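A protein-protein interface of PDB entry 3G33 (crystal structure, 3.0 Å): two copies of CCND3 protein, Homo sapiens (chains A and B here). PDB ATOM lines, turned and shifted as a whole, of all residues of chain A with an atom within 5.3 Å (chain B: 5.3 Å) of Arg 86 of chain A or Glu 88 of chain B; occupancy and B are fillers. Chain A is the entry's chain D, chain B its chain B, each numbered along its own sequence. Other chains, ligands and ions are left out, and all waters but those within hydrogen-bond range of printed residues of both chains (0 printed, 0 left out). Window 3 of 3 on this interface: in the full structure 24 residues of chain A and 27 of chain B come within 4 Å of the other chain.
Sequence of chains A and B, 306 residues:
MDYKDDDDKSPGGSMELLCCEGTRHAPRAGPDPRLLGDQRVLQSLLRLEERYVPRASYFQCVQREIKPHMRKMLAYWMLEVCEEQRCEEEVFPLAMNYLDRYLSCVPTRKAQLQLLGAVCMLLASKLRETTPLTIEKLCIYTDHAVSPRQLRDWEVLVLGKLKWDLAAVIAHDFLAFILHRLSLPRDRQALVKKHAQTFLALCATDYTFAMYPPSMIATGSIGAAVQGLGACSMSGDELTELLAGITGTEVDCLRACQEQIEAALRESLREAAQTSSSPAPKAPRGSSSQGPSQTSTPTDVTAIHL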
ATOM      1  N   VAL A  81      -4.434  31.183  -3.674  1.00  0.00           N
ATOM      2  CA  VAL A  81      -5.263  32.329  -4.016  1.00  0.00           C
ATOM      3  C   VAL A  81      -5.750  32.261  -5.458  1.00  0.00           C
ATOM      4  O   VAL A  81      -6.927  32.488  -5.735  1.00  0.00           O
ATOM      5  CB  VAL A  81      -4.509  33.654  -3.796  1.00  0.00           C
ATOM      6  CG1 VAL A  81      -5.299  34.815  -4.377  1.00  0.00           C
ATOM      7  CG2 VAL A  81      -4.241  33.869  -2.314  1.00  0.00           C
ATOM      8  N   CYS A  82      -4.839  31.944  -6.373  1.00  0.00           N
ATOM      9  CA  CYS A  82      -5.172  31.900  -7.791  1.00  0.00           C
ATOM     10  C   CYS A  82      -6.098  30.735  -8.119  1.00  0.00           C
ATOM     11  O   CYS A  82      -7.052  30.887  -8.881  1.00  0.00           O
ATOM     12  CB  CYS A  82      -3.903  31.827  -8.637  1.00  0.00           C
ATOM     13  SG  CYS A  82      -2.820  33.251  -8.427  1.00  0.00           S
ATOM     14  N   GLU A  83      -5.813  29.575  -7.541  1.00  0.00           N
ATOM     15  CA  GLU A  83      -6.664  28.410  -7.728  1.00  0.00           C
ATOM     16  C   GLU A  83      -8.025  28.654  -7.091  1.00  0.00           C
ATOM     17  O   GLU A  83      -9.038  28.123  -7.540  1.00  0.00           O
ATOM     18  CB  GLU A  83      -6.008  27.166  -7.127  1.00  0.00           C
ATOM     19  CG  GLU A  83      -4.760  26.708  -7.865  1.00  0.00           C
ATOM     20  CD  GLU A  83      -5.074  26.083  -9.213  1.00  0.00           C
ATOM     21  OE1 GLU A  83      -6.127  25.417  -9.330  1.00  0.00           O
ATOM     22  OE2 GLU A  83      -4.268  26.251 -10.152  1.00  0.00           O
ATOM     23  N   GLU A  84      -8.037  29.470  -6.041  1.00  0.00           N
ATOM     24  CA  GLU A  84      -9.270  29.807  -5.344  1.00  0.00           C
ATOM     25  C   GLU A  84     -10.113  30.751  -6.195  1.00  0.00           C
ATOM     26  O   GLU A  84     -11.312  30.544  -6.371  1.00  0.00           O
ATOM     27  CB  GLU A  84      -8.957  30.457  -3.994  1.00  0.00           C
ATOM     28  CG  GLU A  84      -9.930  30.096  -2.881  1.00  0.00           C
ATOM     29  CD  GLU A  84      -9.618  28.750  -2.255  1.00  0.00           C
ATOM     30  OE1 GLU A  84      -8.497  28.241  -2.473  1.00  0.00           O
ATOM     31  OE2 GLU A  84     -10.487  28.203  -1.542  1.00  0.00           O
ATOM     32  N   GLN A  85      -9.475  31.791  -6.721  1.00  0.00           N
ATOM     33  CA  GLN A  85     -10.149  32.757  -7.585  1.00  0.00           C
ATOM     34  C   GLN A  85     -10.284  32.252  -9.016  1.00  0.00           C
ATOM     35  O   GLN A  85     -10.787  32.962  -9.887  1.00  0.00           O
ATOM     36  CB  GLN A  85      -9.410  34.099  -7.580  1.00  0.00           C
ATOM     37  CG  GLN A  85     -10.187  35.247  -6.946  1.00  0.00           C
ATOM     38  CD  GLN A  85     -10.613  34.959  -5.521  1.00  0.00           C
ATOM     39  OE1 GLN A  85     -10.311  33.900  -4.971  1.00  0.00           O
ATOM     40  NE2 GLN A  85     -11.319  35.905  -4.914  1.00  0.00           N
ATOM     41  N   ARG A  86      -9.834  31.026  -9.259  1.00  0.00           N
ATOM     42  CA  ARG A  86      -9.897  30.460 -10.600  1.00  0.00           C
ATOM     43  C   ARG A  86      -9.292  31.416 -11.621  1.00  0.00           C
ATOM     44  O   ARG A  86      -9.795  31.553 -12.735  1.00  0.00           O
ATOM     45  CB  ARG A  86     -11.343  30.123 -10.972  1.00  0.00           C
ATOM     46  CG  ARG A  86     -11.763  28.721 -10.572  1.00  0.00           C
ATOM     47  CD  ARG A  86     -11.279  27.708 -11.593  1.00  0.00           C
ATOM     48  NE  ARG A  86     -10.917  26.437 -10.977  1.00  0.00           N
ATOM     49  CZ  ARG A  86      -9.672  26.090 -10.670  1.00  0.00           C
ATOM     50  NH1 ARG A  86      -8.672  26.923 -10.924  1.00  0.00           N
ATOM     51  NH2 ARG A  86      -9.424  24.915 -10.111  1.00  0.00           N
ATOM     52  N   CYS A  87      -8.210  32.079 -11.227  1.00  0.00           N
ATOM     53  CA  CYS A  87      -7.494  32.982 -12.118  1.00  0.00           C
ATOM     54  C   CYS A  87      -7.006  32.237 -13.350  1.00  0.00           C
ATOM     55  O   CYS A  87      -6.899  31.012 -13.342  1.00  0.00           O
ATOM     56  CB  CYS A  87      -6.294  33.601 -11.400  1.00  0.00           C
ATOM     57  SG  CYS A  87      -6.711  34.589  -9.953  1.00  0.00           S
ATOM     58  N   GLU A  88      -6.711  32.982 -14.408  1.00  0.00           N
ATOM     59  CA  GLU A  88      -6.094  32.397 -15.585  1.00  0.00           C
ATOM     60  C   GLU A  88      -4.799  31.710 -15.163  1.00  0.00           C
ATOM     61  O   GLU A  88      -4.046  32.239 -14.347  1.00  0.00           O
ATOM     62  CB  GLU A  88      -5.822  33.473 -16.635  1.00  0.00           C
ATOM     63  CG  GLU A  88      -7.082  34.061 -17.251  1.00  0.00           C
ATOM     64  CD  GLU A  88      -7.744  33.112 -18.228  1.00  0.00           C
ATOM     65  OE1 GLU A  88      -7.022  32.515 -19.054  1.00  0.00           O
ATOM     66  OE2 GLU A  88      -8.982  32.963 -18.174  1.00  0.00           O
ATOM     67  N   GLU A 129      -5.869  39.143 -17.212  1.00  0.00           N
ATOM     68  CA  GLU A 129      -7.230  38.667 -16.967  1.00  0.00           C
ATOM     69  C   GLU A 129      -8.300  39.667 -17.401  1.00  0.00           C
ATOM     70  O   GLU A 129      -8.130  40.878 -17.263  1.00  0.00           O
ATOM     71  CB  GLU A 129      -7.430  38.313 -15.493  1.00  0.00           C
ATOM     72  CG  GLU A 129      -6.630  37.116 -15.020  1.00  0.00           C
ATOM     73  CD  GLU A 129      -7.260  36.440 -13.818  1.00  0.00           C
ATOM     74  OE1 GLU A 129      -8.298  35.766 -13.991  1.00  0.00           O
ATOM     75  OE2 GLU A 129      -6.714  36.575 -12.703  1.00  0.00           O
ATOM     76  N   ARG B  86     -12.503  28.717 -17.621  1.00  0.00           N
ATOM     77  CA  ARG B  86     -12.021  28.651 -16.249  1.00  0.00           C
ATOM     78  C   ARG B  86     -13.168  28.364 -15.288  1.00  0.00           C
ATOM     79  O   ARG B  86     -13.221  28.915 -14.189  1.00  0.00           O
ATOM     80  CB  ARG B  86     -11.314  29.952 -15.865  1.00  0.00           C
ATOM     81  CG  ARG B  86      -9.828  29.955 -16.180  1.00  0.00           C
ATOM     82  CD  ARG B  86      -9.048  29.242 -15.089  1.00  0.00           C
ATOM     83  NE  ARG B  86      -7.898  28.517 -15.617  1.00  0.00           N
ATOM     84  CZ  ARG B  86      -7.903  27.216 -15.891  1.00  0.00           C
ATOM     85  NH1 ARG B  86      -9.000  26.498 -15.682  1.00  0.00           N
ATOM     86  NH2 ARG B  86      -6.814  26.632 -16.370  1.00  0.00           N
ATOM     87  N   CYS B  87     -14.086  27.503 -15.714  1.00  0.00           N
ATOM     88  CA  CYS B  87     -15.204  27.093 -14.875  1.00  0.00           C
ATOM     89  C   CYS B  87     -14.698  26.450 -13.592  1.00  0.00           C
ATOM     90  O   CYS B  87     -13.557  25.995 -13.522  1.00  0.00           O
ATOM     91  CB  CYS B  87     -16.095  26.089 -15.613  1.00  0.00           C
ATOM     92  SG  CYS B  87     -16.846  26.694 -17.134  1.00  0.00           S
ATOM     93  N   GLU B  88     -15.556  26.407 -12.580  1.00  0.00           N
ATOM     94  CA  GLU B  88     -15.246  25.673 -11.365  1.00  0.00           C
ATOM     95  C   GLU B  88     -14.933  24.225 -11.730  1.00  0.00           C
ATOM     96  O   GLU B  88     -15.608  23.627 -12.568  1.00  0.00           O
ATOM     97  CB  GLU B  88     -16.419  25.743 -10.389  1.00  0.00           C
ATOM     98  CG  GLU B  88     -16.663  27.132  -9.822  1.00  0.00           C
ATOM     99  CD  GLU B  88     -15.627  27.521  -8.790  1.00  0.00           C
ATOM    100  OE1 GLU B  88     -15.317  26.682  -7.919  1.00  0.00           O
ATOM    101  OE2 GLU B  88     -15.126  28.664  -8.843  1.00  0.00           O
ATOM    102  N   GLU B  89     -13.903  23.669 -11.105  1.00  0.00           N
ATOM    103  CA  GLU B  89     -13.437  22.323 -11.429  1.00  0.00           C
ATOM    104  C   GLU B  89     -14.547  21.276 -11.405  1.00  0.00           C
ATOM    105  O   GLU B  89     -14.422  20.212 -12.014  1.00  0.00           O
ATOM    106  CB  GLU B  89     -12.314  21.913 -10.473  1.00  0.00           C
ATOM    107  CG  GLU B  89     -10.959  22.508 -10.814  1.00  0.00           C
ATOM    108  CD  GLU B  89     -10.281  21.778 -11.955  1.00  0.00           C
ATOM    109  OE1 GLU B  89     -10.786  20.706 -12.353  1.00  0.00           O
ATOM    110  OE2 GLU B  89      -9.244  22.269 -12.450  1.00  0.00           O
ATOM    111  N   GLU B  90     -15.634  21.581 -10.706  1.00  0.00           N
ATOM    112  CA  GLU B  90     -16.703  20.611 -10.486  1.00  0.00           C
ATOM    113  C   GLU B  90     -17.659  20.489 -11.672  1.00  0.00           C
ATOM    114  O   GLU B  90     -18.273  19.442 -11.877  1.00  0.00           O
ATOM    115  CB  GLU B  90     -17.473  20.977  -9.218  1.00  0.00           C
ATOM    116  CG  GLU B  90     -16.584  21.063  -7.991  1.00  0.00           C
ATOM    117  CD  GLU B  90     -16.869  22.288  -7.149  1.00  0.00           C
ATOM    118  OE1 GLU B  90     -18.048  22.509  -6.797  1.00  0.00           O
ATOM    119  OE2 GLU B  90     -15.910  23.032  -6.842  1.00  0.00           O
ATOM    120  N   VAL B  91     -17.770  21.557 -12.455  1.00  0.00           N
ATOM    121  CA  VAL B  91     -18.715  21.603 -13.568  1.00  0.00           C
ATOM    122  C   VAL B  91     -18.565  20.440 -14.547  1.00  0.00           C
ATOM    123  O   VAL B  91     -19.522  19.704 -14.795  1.00  0.00           O
ATOM    124  CB  VAL B  91     -18.612  22.931 -14.339  1.00  0.00           C
ATOM    125  CG1 VAL B  91     -19.502  22.897 -15.571  1.00  0.00           C
ATOM    126  CG2 VAL B  91     -18.988  24.093 -13.436  1.00  0.00           C
ATOM    127  N   PHE B  92     -17.370  20.276 -15.104  1.00  0.00           N
ATOM    128  CA  PHE B  92     -17.143  19.243 -16.115  1.00  0.00           C
ATOM    129  C   PHE B  92     -17.706  17.877 -15.719  1.00  0.00           C
ATOM    130  O   PHE B  92     -18.600  17.354 -16.386  1.00  0.00           O
ATOM    131  CB  PHE B  92     -15.655  19.126 -16.453  1.00  0.00           C
ATOM    132  CG  PHE B  92     -15.333  17.979 -17.370  1.00  0.00           C
ATOM    133  CD1 PHE B  92     -15.969  17.851 -18.593  1.00  0.00           C
ATOM    134  CD2 PHE B  92     -14.386  17.033 -17.010  1.00  0.00           C
ATOM    135  CE1 PHE B  92     -15.673  16.797 -19.439  1.00  0.00           C
ATOM    136  CE2 PHE B  92     -14.083  15.979 -17.853  1.00  0.00           C
ATOM    137  CZ  PHE B  92     -14.727  15.860 -19.067  1.00  0.00           C
ATOM    138  N   ARG B 128     -23.623  25.254 -10.081  1.00  0.00           N
ATOM    139  CA  ARG B 128     -22.436  25.207  -9.236  1.00  0.00           C
ATOM    140  C   ARG B 128     -21.464  26.376  -9.431  1.00  0.00           C
ATOM    141  O   ARG B 128     -20.358  26.358  -8.895  1.00  0.00           O
ATOM    142  CB  ARG B 128     -21.715  23.872  -9.447  1.00  0.00           C
ATOM    143  CG  ARG B 128     -20.999  23.341  -8.220  1.00  0.00           C
ATOM    144  CD  ARG B 128     -20.621  21.877  -8.402  1.00  0.00           C
ATOM    145  NE  ARG B 128     -21.770  20.986  -8.265  1.00  0.00           N
ATOM    146  CZ  ARG B 128     -21.902  20.078  -7.302  1.00  0.00           C
ATOM    147  NH1 ARG B 128     -20.953  19.931  -6.388  1.00  0.00           N
ATOM    148  NH2 ARG B 128     -22.982  19.311  -7.258  1.00  0.00           N
ATOM    149  N   GLU B 129     -21.872  27.390 -10.188  1.00  0.00           N
ATOM    150  CA  GLU B 129     -21.015  28.556 -10.407  1.00  0.00           C
ATOM    151  C   GLU B 129     -21.697  29.873 -10.047  1.00  0.00           C
ATOM    152  O   GLU B 129     -22.895  30.047 -10.269  1.00  0.00           O
ATOM    153  CB  GLU B 129     -20.525  28.610 -11.854  1.00  0.00           C
ATOM    154  CG  GLU B 129     -19.583  27.487 -12.240  1.00  0.00           C
ATOM    155  CD  GLU B 129     -18.686  27.862 -13.400  1.00  0.00           C
ATOM    156  OE1 GLU B 129     -17.759  28.673 -13.194  1.00  0.00           O
ATOM    157  OE2 GLU B 129     -18.901  27.342 -14.514  1.00  0.00           O
ATOM    158  N   GLN B 197      -6.983  16.843  -9.383  1.00  0.00           N
ATOM    159  CA  GLN B 197      -8.114  17.238 -10.219  1.00  0.00           C
ATOM    160  C   GLN B 197      -7.975  16.818 -11.680  1.00  0.00           C
ATOM    161  O   GLN B 197      -8.970  16.705 -12.392  1.00  0.00           O
ATOM    162  CB  GLN B 197      -8.354  18.746 -10.117  1.00  0.00           C
ATOM    163  CG  GLN B 197      -9.068  19.159  -8.841  1.00  0.00           C
ATOM    164  CD  GLN B 197      -9.081  20.658  -8.638  1.00  0.00           C
ATOM    165  OE1 GLN B 197      -8.202  21.371  -9.125  1.00  0.00           O
ATOM    166  NE2 GLN B 197     -10.080  21.147  -7.909  1.00  0.00           N
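The side-chain carboxylate (OE2) of Glu 89 of chain B lies within salt-bridge range of the guanidinium group (NH2) of Arg 86 of chain A, at 3.5 Å.
The side-chain sulfur (SG) of Cys 87 of chain B sits close to the side-chain carboxylate (OE2) of Glu 129 of chain B. N of Glu 88 of chain B is in hydrogen-bond range of OE1 of Glu 129 of chain B, at 3.2 Å. O of Cys 82 of chain A lies within hydrogen-bond range of N of Cys 87 of chain A, at 2.9 Å. OE1 of Glu 83 of chain A is in salt-bridge range of NH1 of Arg 86 of chain A (3.4 Å). The side-chain sulfur (SG) of Cys 87 of chain A lies close to the side-chain carboxylate (OE2) of Glu 129 of chain A (3.4 Å). The backbone NH (N) of Glu 88 of chain A sits at hydrogen-bond distance from the side-chain carboxylate (OE1) of Glu 129 of chain A.
Arg 86 of chain A touches Arg 86 of chain B. CD of Arg 86 of chain A touches O of Cys 87 of chain B, at 3.4 Å. Glu 88 of chain B touches Arg 86 of chain A. Gln 197 of chain B touches Arg 86 of chain A (OE1 to NH2, 3.9 Å). Cys 87 of chain A touches Arg 86 of chain B (O to CD, 3.3 Å). CG of Arg 86 of chain B touches OE2 of Glu 88 of chain A, at 3.7 Å.
Arg 86 of chain A touches five residues of chain B. Printed residues of chain A within 4 Å of Gln 197 of chain B: Arg 86 (3.9 Å). Of the printed residues of chain A, Glu 89 of chain B touches Arg 86 (2.9 Å). Of the printed residues of chain A, Cys 87 of chain B touches Arg 86 (3.4 Å). Of the printed residues of chain A, Arg 86 of chain B touches Arg 86 (3.4 Å), Cys 87 (3.3 Å) and Glu 88 (3.7 Å). Arg 128 of chain B touches none of the printed residues of chain A. The nearest residue of chain A that does not touch Glu 88 of chain B is Glu 84 of chain A (4.9 Å).
Of the 9 printed residues of chain A, 3 touch a printed residue of chain B. Printed residues of chain A that touch a printed residue of chain B: Arg 86, Cys 87 and Glu 88. Printed residues of chain B that touch a printed residue of chain A: Arg 86, Cys 87, Glu 88, Glu 89 and Gln 197. Along chain B the printed residues that touch a printed residue of chain A span positions 86 to 197. Among the printed residues, Asp or Glu carboxylates within 4 Å of a Lys or Arg side-chain nitrogen of the other chain: Arg 86 of chain A with Glu 89 of chain B (3.5 Å).
Arg 86 of chain B touches its own counterpart, Arg 86 of chain A. Arg 86 of chain A touches Cys 87 of chain B, and with the chains exchanged Cys 87 of chain A touches Arg 86 of chain B. Arg 86 of chain A touches Glu 88 of chain B, and with the chains exchanged Glu 88 of chain A touches Arg 86 of chain B. Of the 7 pairs that touch across the chains among the printed residues, 5 have their exchanged pair printed and touching as well.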
